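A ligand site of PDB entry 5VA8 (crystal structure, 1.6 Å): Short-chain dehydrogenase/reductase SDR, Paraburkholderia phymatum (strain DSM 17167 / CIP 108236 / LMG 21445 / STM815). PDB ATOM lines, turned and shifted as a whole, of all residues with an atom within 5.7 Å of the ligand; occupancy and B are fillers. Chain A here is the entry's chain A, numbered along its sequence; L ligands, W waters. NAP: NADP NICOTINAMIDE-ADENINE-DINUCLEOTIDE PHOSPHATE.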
ATOM      1  N   CYS A  21      11.629 -18.054  24.329  1.00  0.00           N
ATOM      2  CA  CYS A  21      12.068 -19.410  23.980  1.00  0.00           C
ATOM      3  C   CYS A  21      13.454 -19.421  23.346  1.00  0.00           C
ATOM      4  O   CYS A  21      13.811 -18.529  22.567  1.00  0.00           O
ATOM      5  CB  CYS A  21      11.074 -20.048  23.011  1.00  0.00           C
ATOM      6  SG  CYS A  21       9.427 -20.225  23.678  1.00  0.00           S
ATOM      7  N   ALA A  22      14.220 -20.471  23.653  1.00  0.00           N
ATOM      8  CA  ALA A  22      15.491 -20.744  22.972  1.00  0.00           C
ATOM      9  C   ALA A  22      16.425 -19.545  23.098  1.00  0.00           C
ATOM     10  O   ALA A  22      16.838 -18.918  22.116  1.00  0.00           O
ATOM     11  CB  ALA A  22      15.226 -21.146  21.520  1.00  0.00           C
ATOM     12  N   ALA A  23      16.757 -19.230  24.351  1.00  0.00           N
ATOM     13  CA  ALA A  23      17.238 -17.888  24.654  1.00  0.00           C
ATOM     14  C   ALA A  23      18.444 -17.874  25.585  1.00  0.00           C
ATOM     15  O   ALA A  23      18.713 -16.843  26.222  1.00  0.00           O
ATOM     16  CB  ALA A  23      16.095 -17.041  25.242  1.00  0.00           C
ATOM     17  N   SER A  24      19.203 -18.966  25.688  1.00  0.00           N
ATOM     18  CA  SER A  24      20.461 -18.853  26.413  1.00  0.00           C
ATOM     19  C   SER A  24      21.557 -18.242  25.555  1.00  0.00           C
ATOM     20  O   SER A  24      22.568 -17.787  26.098  1.00  0.00           O
ATOM     21  CB  SER A  24      20.893 -20.222  26.962  1.00  0.00           C
ATOM     22  OG  SER A  24      21.336 -21.095  25.932  1.00  0.00           O
ATOM     23  N   LYS A  25      21.363 -18.209  24.225  1.00  0.00           N
ATOM     24  CA  LYS A  25      22.342 -17.680  23.281  1.00  0.00           C
ATOM     25  C   LYS A  25      21.616 -16.953  22.164  1.00  0.00           C
ATOM     26  O   LYS A  25      20.415 -17.105  21.964  1.00  0.00           O
ATOM     27  CB  LYS A  25      23.203 -18.810  22.664  1.00  0.00           C
ATOM     28  CG  LYS A  25      23.887 -19.697  23.699  1.00  0.00           C
ATOM     29  CD  LYS A  25      24.372 -20.995  23.059  1.00  0.00           C
ATOM     30  CE  LYS A  25      25.262 -20.724  21.872  1.00  0.00           C
ATOM     31  NZ  LYS A  25      25.749 -21.976  21.210  1.00  0.00           N
ATOM     32  N   GLY A  26      22.389 -16.157  21.417  1.00  0.00           N
ATOM     33  CA  GLY A  26      21.971 -15.696  20.090  1.00  0.00           C
ATOM     34  C   GLY A  26      20.807 -14.716  20.122  1.00  0.00           C
ATOM     35  O   GLY A  26      20.675 -13.880  21.023  1.00  0.00           O
ATOM     36  N   LEU A  27      19.960 -14.830  19.094  1.00  0.00           N
ATOM     37  CA  LEU A  27      18.837 -13.905  18.945  1.00  0.00           C
ATOM     38  C   LEU A  27      17.870 -13.996  20.110  1.00  0.00           C
ATOM     39  O   LEU A  27      17.348 -12.968  20.579  1.00  0.00           O
ATOM     40  CB  LEU A  27      18.096 -14.169  17.636  1.00  0.00           C
ATOM     41  CG  LEU A  27      18.946 -14.049  16.387  1.00  0.00           C
ATOM     42  CD1 LEU A  27      18.103 -14.329  15.178  1.00  0.00           C
ATOM     43  CD2 LEU A  27      19.590 -12.674  16.307  1.00  0.00           C
ATOM     44  N   GLY A  28      17.588 -15.211  20.589  1.00  0.00           N
ATOM     45  CA  GLY A  28      16.699 -15.341  21.724  1.00  0.00           C
ATOM     46  C   GLY A  28      17.251 -14.662  22.962  1.00  0.00           C
ATOM     47  O   GLY A  28      16.536 -13.943  23.655  1.00  0.00           O
ATOM     48  N   VAL A  45      14.279 -20.125  28.166  1.00  0.00           N
ATOM     49  CA  VAL A  45      14.210 -21.569  27.928  1.00  0.00           C
ATOM     50  C   VAL A  45      15.366 -21.975  27.033  1.00  0.00           C
ATOM     51  O   VAL A  45      15.609 -21.340  25.990  1.00  0.00           O
ATOM     52  CB  VAL A  45      12.861 -21.955  27.278  1.00  0.00           C
ATOM     53  CG1 VAL A  45      12.837 -23.433  26.994  1.00  0.00           C
ATOM     54  CG2 VAL A  45      11.682 -21.546  28.175  1.00  0.00           C
ATOM     55  N   ALA A  46      16.076 -23.042  27.418  1.00  0.00           N
ATOM     56  CA  ALA A  46      17.073 -23.652  26.552  1.00  0.00           C
ATOM     57  C   ALA A  46      17.286 -25.087  27.019  1.00  0.00           C
ATOM     58  O   ALA A  46      16.909 -25.451  28.136  1.00  0.00           O
ATOM     59  CB  ALA A  46      18.389 -22.879  26.552  1.00  0.00           C
ATOM     60  N   ARG A  47      17.911 -25.891  26.167  1.00  0.00           N
ATOM     61  CA  ARG A  47      18.068 -27.304  26.492  1.00  0.00           C
ATOM     62  C   ARG A  47      19.233 -27.543  27.450  1.00  0.00           C
ATOM     63  O   ARG A  47      19.124 -28.378  28.361  1.00  0.00           O
ATOM     64  CB  ARG A  47      18.255 -28.121  25.218  1.00  0.00           C
ATOM     65  CG  ARG A  47      17.013 -28.127  24.324  1.00  0.00           C
ATOM     66  CD  ARG A  47      17.319 -28.659  22.934  1.00  0.00           C
ATOM     67  NE  ARG A  47      18.315 -27.836  22.258  1.00  0.00           N
ATOM     68  CZ  ARG A  47      18.709 -28.026  21.006  1.00  0.00           C
ATOM     69  NH1 ARG A  47      18.172 -29.002  20.283  1.00  0.00           N
ATOM     70  NH2 ARG A  47      19.642 -27.246  20.466  1.00  0.00           N
ATOM     71  N   THR A  48      20.345 -26.836  27.275  1.00  0.00           N
ATOM     72  CA  THR A  48      21.571 -27.190  27.997  1.00  0.00           C
ATOM     73  C   THR A  48      21.709 -26.347  29.250  1.00  0.00           C
ATOM     74  O   THR A  48      21.804 -25.112  29.148  1.00  0.00           O
ATOM     75  CB  THR A  48      22.777 -27.005  27.088  1.00  0.00           C
ATOM     76  OG1 THR A  48      22.487 -27.545  25.786  1.00  0.00           O
ATOM     77  CG2 THR A  48      23.983 -27.730  27.659  1.00  0.00           C
ATOM     78  N   CYS A  72      14.740 -27.210  28.991  1.00  0.00           N
ATOM     79  CA  CYS A  72      13.875 -28.136  28.283  1.00  0.00           C
ATOM     80  C   CYS A  72      14.007 -27.914  26.788  1.00  0.00           C
ATOM     81  O   CYS A  72      14.495 -26.869  26.336  1.00  0.00           O
ATOM     82  CB  CYS A  72      12.410 -27.985  28.698  1.00  0.00           C
ATOM     83  SG  CYS A  72      11.673 -26.473  28.036  1.00  0.00           S
ATOM     84  N   ASP A  73      13.564 -28.920  26.033  1.00  0.00           N
ATOM     85  CA  ASP A  73      13.393 -28.830  24.592  1.00  0.00           C
ATOM     86  C   ASP A  73      11.999 -28.271  24.336  1.00  0.00           C
ATOM     87  O   ASP A  73      10.997 -28.943  24.611  1.00  0.00           O
ATOM     88  CB  ASP A  73      13.562 -30.234  23.989  1.00  0.00           C
ATOM     89  CG  ASP A  73      13.473 -30.247  22.478  1.00  0.00           C
ATOM     90  OD1 ASP A  73      12.929 -29.302  21.873  1.00  0.00           O
ATOM     91  OD2 ASP A  73      13.928 -31.252  21.890  1.00  0.00           O
ATOM     92  N   ILE A  74      11.940 -27.030  23.866  1.00  0.00           N
ATOM     93  CA  ILE A  74      10.654 -26.352  23.701  1.00  0.00           C
ATOM     94  C   ILE A  74       9.828 -26.950  22.570  1.00  0.00           C
ATOM     95  O   ILE A  74       8.638 -26.647  22.462  1.00  0.00           O
ATOM     96  CB  ILE A  74      10.904 -24.842  23.487  1.00  0.00           C
ATOM     97  CG1 ILE A  74       9.644 -24.020  23.760  1.00  0.00           C
ATOM     98  CG2 ILE A  74      11.417 -24.563  22.063  1.00  0.00           C
ATOM     99  CD1 ILE A  74       9.162 -24.107  25.193  1.00  0.00           C
ATOM    100  N   THR A  75      10.429 -27.815  21.750  1.00  0.00           N
ATOM    101  CA  THR A  75       9.718 -28.386  20.612  1.00  0.00           C
ATOM    102  C   THR A  75       9.026 -29.700  20.956  1.00  0.00           C
ATOM    103  O   THR A  75       8.593 -30.414  20.045  1.00  0.00           O
ATOM    104  CB  THR A  75      10.651 -28.573  19.400  1.00  0.00           C
ATOM    105  OG1 THR A  75      11.598 -29.639  19.615  1.00  0.00           O
ATOM    106  CG2 THR A  75      11.382 -27.260  19.080  1.00  0.00           C
ATOM    107  N   ASN A  96      10.637 -19.166  19.369  1.00  0.00           N
ATOM    108  CA  ASN A  96      11.972 -19.398  18.848  1.00  0.00           C
ATOM    109  C   ASN A  96      12.333 -20.843  19.165  1.00  0.00           C
ATOM    110  O   ASN A  96      11.859 -21.409  20.154  1.00  0.00           O
ATOM    111  CB  ASN A  96      12.985 -18.435  19.479  1.00  0.00           C
ATOM    112  CG  ASN A  96      14.355 -18.489  18.823  1.00  0.00           C
ATOM    113  OD1 ASN A  96      14.456 -18.666  17.604  1.00  0.00           O
ATOM    114  ND2 ASN A  96      15.394 -18.289  19.622  1.00  0.00           N
ATOM    115  N   ALA A  97      13.173 -21.424  18.326  1.00  0.00           N
ATOM    116  CA  ALA A  97      13.713 -22.771  18.487  1.00  0.00           C
ATOM    117  C   ALA A  97      14.810 -22.935  17.447  1.00  0.00           C
ATOM    118  O   ALA A  97      14.900 -22.152  16.494  1.00  0.00           O
ATOM    119  CB  ALA A  97      12.648 -23.867  18.293  1.00  0.00           C
ATOM    120  N   GLY A  98      15.655 -23.940  17.645  1.00  0.00           N
ATOM    121  CA  GLY A  98      16.697 -24.196  16.664  1.00  0.00           C
ATOM    122  C   GLY A  98      16.103 -24.502  15.300  1.00  0.00           C
ATOM    123  O   GLY A  98      15.057 -25.136  15.189  1.00  0.00           O
ATOM    124  N   GLY A  99      16.800 -24.046  14.256  1.00  0.00           N
ATOM    125  CA  GLY A  99      16.334 -24.206  12.903  1.00  0.00           C
ATOM    126  C   GLY A  99      16.758 -25.530  12.296  1.00  0.00           C
ATOM    127  O   GLY A  99      17.541 -26.294  12.875  1.00  0.00           O
ATOM    128  N   PRO A 100      16.242 -25.820  11.107  1.00  0.00           N
ATOM    129  CA  PRO A 100      16.480 -27.142  10.494  1.00  0.00           C
ATOM    130  C   PRO A 100      17.850 -27.223   9.851  1.00  0.00           C
ATOM    131  O   PRO A 100      18.505 -26.197   9.600  1.00  0.00           O
ATOM    132  CB  PRO A 100      15.363 -27.258   9.448  1.00  0.00           C
ATOM    133  CG  PRO A 100      15.040 -25.828   9.081  1.00  0.00           C
ATOM    134  CD  PRO A 100      15.303 -25.003  10.328  1.00  0.00           C
ATOM    135  N   ASN A 120       9.592 -25.442  14.050  1.00  0.00           N
ATOM    136  CA  ASN A 120       9.555 -24.068  13.583  1.00  0.00           C
ATOM    137  C   ASN A 120       8.185 -23.631  13.096  1.00  0.00           C
ATOM    138  O   ASN A 120       8.032 -22.489  12.623  1.00  0.00           O
ATOM    139  CB  ASN A 120      10.605 -23.857  12.488  1.00  0.00           C
ATOM    140  CG  ASN A 120      11.996 -24.302  12.935  1.00  0.00           C
ATOM    141  OD1 ASN A 120      12.613 -25.170  12.319  1.00  0.00           O
ATOM    142  ND2 ASN A 120      12.491 -23.713  14.030  1.00  0.00           N
ATOM    143  N   ILE A 146      10.195 -15.405  16.036  1.00  0.00           N
ATOM    144  CA  ILE A 146      11.456 -15.297  15.295  1.00  0.00           C
ATOM    145  C   ILE A 146      11.400 -16.288  14.154  1.00  0.00           C
ATOM    146  O   ILE A 146      11.318 -17.496  14.382  1.00  0.00           O
ATOM    147  CB  ILE A 146      12.659 -15.567  16.212  1.00  0.00           C
ATOM    148  CG1 ILE A 146      12.738 -14.534  17.329  1.00  0.00           C
ATOM    149  CG2 ILE A 146      13.952 -15.619  15.371  1.00  0.00           C
ATOM    150  CD1 ILE A 146      13.871 -14.822  18.320  1.00  0.00           C
ATOM    151  N   THR A 147      11.445 -15.783  12.920  1.00  0.00           N
ATOM    152  CA  THR A 147      11.351 -16.661  11.756  1.00  0.00           C
ATOM    153  C   THR A 147      12.648 -16.534  10.965  1.00  0.00           C
ATOM    154  O   THR A 147      13.707 -16.892  11.481  1.00  0.00           O
ATOM    155  CB  THR A 147      10.099 -16.386  10.916  1.00  0.00           C
ATOM    156  OG1 THR A 147      10.085 -15.044  10.405  1.00  0.00           O
ATOM    157  CG2 THR A 147       8.838 -16.614  11.778  1.00  0.00           C
ATOM    158  N   SER A 148      12.583 -16.010   9.740  1.00  0.00           N
ATOM    159  CA  SER A 148      13.745 -16.002   8.853  1.00  0.00           C
ATOM    160  C   SER A 148      13.424 -15.205   7.606  1.00  0.00           C
ATOM    161  O   SER A 148      12.267 -15.159   7.174  1.00  0.00           O
ATOM    162  CB  SER A 148      14.148 -17.431   8.444  1.00  0.00           C
ATOM    163  OG  SER A 148      15.264 -17.386   7.562  1.00  0.00           O
ATOM    164  N   SER A 149      14.466 -14.638   6.998  1.00  0.00           N
ATOM    165  CA  SER A 149      14.320 -14.094   5.652  1.00  0.00           C
ATOM    166  C   SER A 149      13.855 -15.148   4.653  1.00  0.00           C
ATOM    167  O   SER A 149      13.387 -14.789   3.573  1.00  0.00           O
ATOM    168  CB  SER A 149      15.653 -13.501   5.184  1.00  0.00           C
ATOM    169  OG  SER A 149      16.575 -14.542   4.896  1.00  0.00           O
ATOM    170  N   ARG A 165       8.823 -22.403   7.995  1.00  0.00           N
ATOM    171  CA  ARG A 165       8.595 -21.078   8.544  1.00  0.00           C
ATOM    172  C   ARG A 165       7.577 -20.305   7.739  1.00  0.00           C
ATOM    173  O   ARG A 165       6.876 -19.448   8.304  1.00  0.00           O
ATOM    174  CB  ARG A 165       9.912 -20.301   8.623  1.00  0.00           C
ATOM    175  CG  ARG A 165      10.943 -21.043   9.471  1.00  0.00           C
ATOM    176  CD  ARG A 165      12.103 -20.108   9.706  1.00  0.00           C
ATOM    177  NE  ARG A 165      13.325 -20.731  10.190  1.00  0.00           N
ATOM    178  CZ  ARG A 165      13.709 -20.793  11.468  1.00  0.00           C
ATOM    179  NH1 ARG A 165      12.910 -20.347  12.444  1.00  0.00           N
ATOM    180  NH2 ARG A 165      14.902 -21.302  11.748  1.00  0.00           N
ATOM    181  N   PRO A 191      14.978 -12.451  10.680  1.00  0.00           N
ATOM    182  CA  PRO A 191      16.398 -12.097  10.577  1.00  0.00           C
ATOM    183  C   PRO A 191      16.956 -12.416   9.205  1.00  0.00           C
ATOM    184  O   PRO A 191      16.665 -13.475   8.625  1.00  0.00           O
ATOM    185  CB  PRO A 191      17.081 -12.953  11.653  1.00  0.00           C
ATOM    186  CG  PRO A 191      16.014 -13.787  12.281  1.00  0.00           C
ATOM    187  CD  PRO A 191      14.760 -13.678  11.465  1.00  0.00           C
ATOM    188  N   GLY A 192      17.777 -11.491   8.684  1.00  0.00           N
ATOM    189  CA  GLY A 192      18.774 -11.819   7.689  1.00  0.00           C
ATOM    190  C   GLY A 192      19.927 -12.503   8.389  1.00  0.00           C
ATOM    191  O   GLY A 192      19.701 -13.265   9.330  1.00  0.00           O
ATOM    192  N   ILE A 193      21.180 -12.260   7.996  1.00  0.00           N
ATOM    193  CA  ILE A 193      22.271 -12.966   8.647  1.00  0.00           C
ATOM    194  C   ILE A 193      22.718 -12.186   9.880  1.00  0.00           C
ATOM    195  O   ILE A 193      23.001 -10.980   9.820  1.00  0.00           O
ATOM    196  CB  ILE A 193      23.440 -13.221   7.674  1.00  0.00           C
ATOM    197  CG1 ILE A 193      24.537 -14.013   8.400  1.00  0.00           C
ATOM    198  CG2 ILE A 193      23.972 -11.947   7.055  1.00  0.00           C
ATOM    199  CD1 ILE A 193      25.639 -14.540   7.482  1.00  0.00           C
ATOM    200  N   PHE A 194      22.741 -12.879  11.027  1.00  0.00           N
ATOM    201  CA  PHE A 194      23.118 -12.296  12.309  1.00  0.00           C
ATOM    202  C   PHE A 194      24.309 -13.039  12.886  1.00  0.00           C
ATOM    203  O   PHE A 194      24.434 -14.255  12.743  1.00  0.00           O
ATOM    204  CB  PHE A 194      21.942 -12.327  13.285  1.00  0.00           C
ATOM    205  CG  PHE A 194      21.022 -11.144  13.130  1.00  0.00           C
ATOM    206  CD1 PHE A 194      21.039 -10.116  14.070  1.00  0.00           C
ATOM    207  CD2 PHE A 194      20.198 -11.032  12.021  1.00  0.00           C
ATOM    208  CE1 PHE A 194      20.230  -9.012  13.919  1.00  0.00           C
ATOM    209  CE2 PHE A 194      19.384  -9.922  11.858  1.00  0.00           C
ATOM    210  CZ  PHE A 194      19.391  -8.910  12.812  1.00  0.00           C
ATOM    211  N   ASP A 195      25.183 -12.276  13.556  1.00  0.00           N
ATOM    212  CA  ASP A 195      26.474 -12.741  14.049  1.00  0.00           C
ATOM    213  C   ASP A 195      26.275 -13.558  15.317  1.00  0.00           C
ATOM    214  O   ASP A 195      26.491 -13.091  16.441  1.00  0.00           O
ATOM    215  CB  ASP A 195      27.382 -11.541  14.289  1.00  0.00           C
ATOM    216  CG  ASP A 195      28.839 -11.907  14.328  1.00  0.00           C
ATOM    217  OD1 ASP A 195      29.152 -13.102  14.123  1.00  0.00           O
ATOM    218  OD2 ASP A 195      29.665 -11.002  14.551  1.00  0.00           O
ATOM    219  N   THR A 196      25.846 -14.814  15.149  1.00  0.00           N
ATOM    220  CA  THR A 196      25.649 -15.748  16.266  1.00  0.00           C
ATOM    221  C   THR A 196      26.462 -17.020  16.021  1.00  0.00           C
ATOM    222  O   THR A 196      27.086 -17.196  14.975  1.00  0.00           O
ATOM    223  CB  THR A 196      24.182 -16.131  16.446  1.00  0.00           C
ATOM    224  OG1 THR A 196      23.801 -16.978  15.355  1.00  0.00           O
ATOM    225  CG2 THR A 196      23.282 -14.905  16.497  1.00  0.00           C
ATOM    226  N   ASP A 197      26.410 -17.924  17.001  1.00  0.00           N
ATOM    227  CA  ASP A 197      27.079 -19.206  16.843  1.00  0.00           C
ATOM    228  C   ASP A 197      26.512 -20.020  15.692  1.00  0.00           C
ATOM    229  O   ASP A 197      27.216 -20.895  15.161  1.00  0.00           O
ATOM    230  CB  ASP A 197      26.991 -20.017  18.130  1.00  0.00           C
ATOM    231  CG  ASP A 197      27.932 -19.526  19.208  1.00  0.00           C
ATOM    232  OD1 ASP A 197      28.755 -18.624  18.938  1.00  0.00           O
ATOM    233  OD2 ASP A 197      27.841 -20.046  20.337  1.00  0.00           O
ATOM    234  N   ARG A 198      25.259 -19.767  15.293  1.00  0.00           N
ATOM    235  CA  ARG A 198      24.650 -20.546  14.212  1.00  0.00           C
ATOM    236  C   ARG A 198      25.400 -20.363  12.905  1.00  0.00           C
ATOM    237  O   ARG A 198      25.598 -21.326  12.158  1.00  0.00           O
ATOM    238  CB  ARG A 198      23.176 -20.158  14.056  1.00  0.00           C
ATOM    239  N   ILE A 199      25.823 -19.132  12.605  1.00  0.00           N
ATOM    240  CA  ILE A 199      26.458 -18.890  11.318  1.00  0.00           C
ATOM    241  C   ILE A 199      27.934 -19.250  11.325  1.00  0.00           C
ATOM    242  O   ILE A 199      28.539 -19.394  10.252  1.00  0.00           O
ATOM    243  CB  ILE A 199      26.296 -17.438  10.844  1.00  0.00           C
ATOM    244  CG1 ILE A 199      27.212 -16.517  11.637  1.00  0.00           C
ATOM    245  CG2 ILE A 199      24.843 -17.012  10.977  1.00  0.00           C
ATOM    246  CD1 ILE A 199      27.301 -15.125  11.050  1.00  0.00           C
HETATM  247  PA  NAP L   1      22.016 -19.741  18.416  1.00  0.00           P
HETATM  248  O1A NAP L   1      22.955 -18.621  18.630  1.00  0.00           O
HETATM  249  O2A NAP L   1      22.646 -21.095  18.175  1.00  0.00           O
HETATM  250  O5B NAP L   1      21.063 -19.787  19.697  1.00  0.00           O
HETATM  251  C5B NAP L   1      20.034 -20.780  19.764  1.00  0.00           C
HETATM  252  C4B NAP L   1      19.502 -20.788  21.173  1.00  0.00           C
HETATM  253  O4B NAP L   1      18.303 -21.579  21.212  1.00  0.00           O
HETATM  254  C3B NAP L   1      20.437 -21.412  22.216  1.00  0.00           C
HETATM  255  O3B NAP L   1      20.220 -20.802  23.474  1.00  0.00           O
HETATM  256  C2B NAP L   1      19.967 -22.861  22.222  1.00  0.00           C
HETATM  257  O2B NAP L   1      20.422 -23.503  23.429  1.00  0.00           O
HETATM  258  C1B NAP L   1      18.457 -22.655  22.124  1.00  0.00           C
HETATM  259  N9A NAP L   1      17.710 -23.778  21.590  1.00  0.00           N
HETATM  260  C8A NAP L   1      17.869 -24.352  20.359  1.00  0.00           C
HETATM  261  N7A NAP L   1      16.988 -25.300  20.090  1.00  0.00           N
HETATM  262  C5A NAP L   1      16.202 -25.352  21.230  1.00  0.00           C
HETATM  263  C6A NAP L   1      15.106 -26.154  21.598  1.00  0.00           C
HETATM  264  N6A NAP L   1      14.581 -27.092  20.794  1.00  0.00           N
HETATM  265  N1A NAP L   1      14.567 -25.966  22.815  1.00  0.00           N
HETATM  266  C2A NAP L   1      15.087 -25.023  23.607  1.00  0.00           C
HETATM  267  N3A NAP L   1      16.116 -24.206  23.379  1.00  0.00           N
HETATM  268  C4A NAP L   1      16.640 -24.423  22.173  1.00  0.00           C
HETATM  269  O3  NAP L   1      21.047 -19.445  17.174  1.00  0.00           O
HETATM  270  PN  NAP L   1      20.430 -18.096  16.574  1.00  0.00           P
HETATM  271  O1N NAP L   1      20.053 -17.191  17.673  1.00  0.00           O
HETATM  272  O2N NAP L   1      21.362 -17.601  15.533  1.00  0.00           O
HETATM  273  O5D NAP L   1      19.132 -18.691  15.860  1.00  0.00           O
HETATM  274  C5D NAP L   1      17.844 -18.630  16.490  1.00  0.00           C
HETATM  275  C4D NAP L   1      16.838 -19.013  15.426  1.00  0.00           C
HETATM  276  O4D NAP L   1      16.868 -18.008  14.378  1.00  0.00           O
HETATM  277  C3D NAP L   1      17.091 -20.353  14.730  1.00  0.00           C
HETATM  278  O3D NAP L   1      15.854 -20.991  14.392  1.00  0.00           O
HETATM  279  C2D NAP L   1      17.816 -19.932  13.454  1.00  0.00           C
HETATM  280  O2D NAP L   1      17.716 -20.855  12.382  1.00  0.00           O
HETATM  281  C1D NAP L   1      17.045 -18.647  13.150  1.00  0.00           C
HETATM  282  N1N NAP L   1      17.765 -17.714  12.247  1.00  0.00           N
HETATM  283  C2N NAP L   1      19.033 -17.374  12.496  1.00  0.00           C
HETATM  284  C3N NAP L   1      19.674 -16.450  11.685  1.00  0.00           C
HETATM  285  C7N NAP L   1      21.082 -15.977  11.873  1.00  0.00           C
HETATM  286  O7N NAP L   1      21.691 -15.525  10.886  1.00  0.00           O
HETATM  287  N7N NAP L   1      21.662 -16.182  13.051  1.00  0.00           N
HETATM  288  C4N NAP L   1      18.931 -15.852  10.668  1.00  0.00           C
HETATM  289  C5N NAP L   1      17.628 -16.242  10.428  1.00  0.00           C
HETATM  290  C6N NAP L   1      17.055 -17.196  11.227  1.00  0.00           C
HETATM  291  P2B NAP L   1      20.470 -25.114  23.566  1.00  0.00           P
HETATM  292  O1X NAP L   1      19.057 -25.572  23.617  1.00  0.00           O
HETATM  293  O2X NAP L   1      21.222 -25.663  22.351  1.00  0.00           O
HETATM  294  O3X NAP L   1      21.253 -25.353  24.872  1.00  0.00           O
HETATM  295  O   HOH W   1      19.363 -22.945  14.085  1.00  0.00           O
HETATM  296  O   HOH W   2      23.794 -22.636  19.769  1.00  0.00           O
HETATM  297  O   HOH W   3      22.174 -24.764  19.913  1.00  0.00           O
HETATM  298  O   HOH W   4      21.770 -23.603  26.788  1.00  0.00           O
HETATM  299  O   HOH W   5      24.134 -25.014  24.590  1.00  0.00           O
HETATM  300  O   HOH W   6      15.621 -30.257  19.925  1.00  0.00           O
HETATM  301  O   HOH W   7      19.881 -22.007  16.508  1.00  0.00           O
HETATM  302  O   HOH W   8      22.123 -28.364  22.625  1.00  0.00           O
HETATM  303  O   HOH W   9      18.411 -23.382  10.209  1.00  0.00           O
HETATM  304  O   HOH W  10      20.433 -22.048  11.464  1.00  0.00           O
HETATM  305  O   HOH W  11      18.384 -17.798  19.710  1.00  0.00           O
HETATM  306  O   HOH W  12      20.213 -24.297  18.067  1.00  0.00           O
HETATM  307  O   HOH W  13      14.978 -27.040  17.574  1.00  0.00           O
HETATM  308  O   HOH W  14      23.941 -22.703  16.542  1.00  0.00           O
HETATM  309  O   HOH W  15      25.139 -17.570  19.606  1.00  0.00           O
HETATM  310  O   HOH W  16      12.958 -19.426  15.358  1.00  0.00           O
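An oxygen (O7N) of the ligand sits at hydrogen-bond distance from the backbone NH (N) of Phe 194. O1X of the ligand lies within hydrogen-bond range of N of Arg 47 (2.8 Å). A nitrogen (N7A) of the ligand is in hydrogen-bond range of the backbone NH (N) of Gly 98, at 3.1 Å. N of Ile 74 is in hydrogen-bond range of N1A of the ligand (3.0 Å). The backbone NH of Lys 25 sits at hydrogen-bond distance from an oxygen (O3B) of the ligand, 2.9 Å away. The side-chain hydroxyl (OG1) of Thr 48 sits at hydrogen-bond distance from an oxygen (O3X) of the ligand, 2.7 Å away. The side-chain hydroxyl (OG) of Ser 24 lies within hydrogen-bond range of an oxygen (O3B) of the ligand, 2.7 Å away. N7N of the ligand is in hydrogen-bond range of O of Phe 194 (3.4 Å). O3D of the ligand is in hydrogen-bond range of NH2 of Arg 165. O3B of the ligand lies within hydrogen-bond range of N of Ser 24 (3.1 Å). The backbone carbonyl oxygen (O) of Ala 97 is in hydrogen-bond range of an oxygen (O3D) of the ligand (2.6 Å). An oxygen (O3X) of the ligand sits at hydrogen-bond distance from the backbone NH (N) of Thr 48 (3.0 Å). N of Gly 99 is in hydrogen-bond range of O3D of the ligand (3.2 Å). The side-chain hydroxyl of Thr 196 lies within hydrogen-bond range of an oxygen (O2N) of the ligand, at 2.5 Å. N of Leu 27 is in hydrogen-bond range of O1N of the ligand (2.8 Å). OD1 of Asp 73 lies within hydrogen-bond range of N6A of the ligand (3.0 Å). The guanidinium group of Arg 47 lies within salt-bridge range of an oxygen (O1X) of the ligand, at 2.7 Å.
Water W2 bridges O2A of the ligand (2.5 Å) and NZ of Lys 25 (2.5 Å). Water W15 bridges an oxygen (O1A) of the ligand (2.6 Å) and the backbone NH of Asp 197 (2.9 Å). Water W14 lies within hydrogen-bond range of O2A of the ligand (2.6 Å) and N of Arg 198 (3.5 Å). Water W5 lies within hydrogen-bond range of an oxygen (O3X) of the ligand and the side-chain hydroxyl (OG1) of Thr 48. Water W1 bridges the backbone NH of Gly 99 (2.8 Å) and an oxygen (O2D) of the ligand (3.2 Å). Water W13 lies within hydrogen-bond range of O of Gly 98 and N6A of the ligand.
O4B of the ligand sits close to O of Ala 22. The backbone carbonyl oxygen (O) of Gly 192 lies close to an oxygen (O7N) of the ligand, at 3.4 Å. Merely in contact with the ligand: Ala 23 (3.9 Å), Gly 26 (3.4 Å), Val 45 (3.9 Å), Ala 46 (3.4 Å), Cys 72 (3.3 Å), Thr 75 (3.6 Å), Asn 96 (3.2 Å), Ile 146 (3.9 Å), Thr 147 (3.4 Å), Ser 148 (3.9 Å), Pro 191 (3.4 Å), Ile 193 (3.4 Å), Asp 197 (3.9 Å), Arg 198 (3.5 Å) and Ile 199 (3.5 Å). Hydrophobic or aromatic side chains that line the ligand: Ala 22, Leu 27, Ala 46, Ile 74, Ile 146, Pro 191, Phe 194 and Ile 199.
OD1 of Asp 73 lies within hydrogen-bond range of OG1 of Thr 75, 2.6 Å away. The backbone carbonyl oxygen (O) of Val 45 is in hydrogen-bond range of the backbone NH (N) of Ala 23, 2.9 Å away. The backbone carbonyl oxygen of Pro 191 sits at hydrogen-bond distance from the backbone NH of Ser 149 (3.0 Å). NZ of Lys 25 is in salt-bridge range of OD2 of Asp 197 (3.0 Å). The backbone carbonyl oxygen (O) of Ala 46 is in hydrogen-bond range of the backbone NH (N) of Cys 72 (2.9 Å). The side-chain amide nitrogen (ND2) of Asn 96 sits close to the backbone carbonyl oxygen (O) of Cys 21 (3.4 Å). O of Ala 22 is in hydrogen-bond range of ND2 of Asn 96. The backbone NH of Arg 198 lies close to the side-chain hydroxyl of Thr 196 (3.1 Å).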
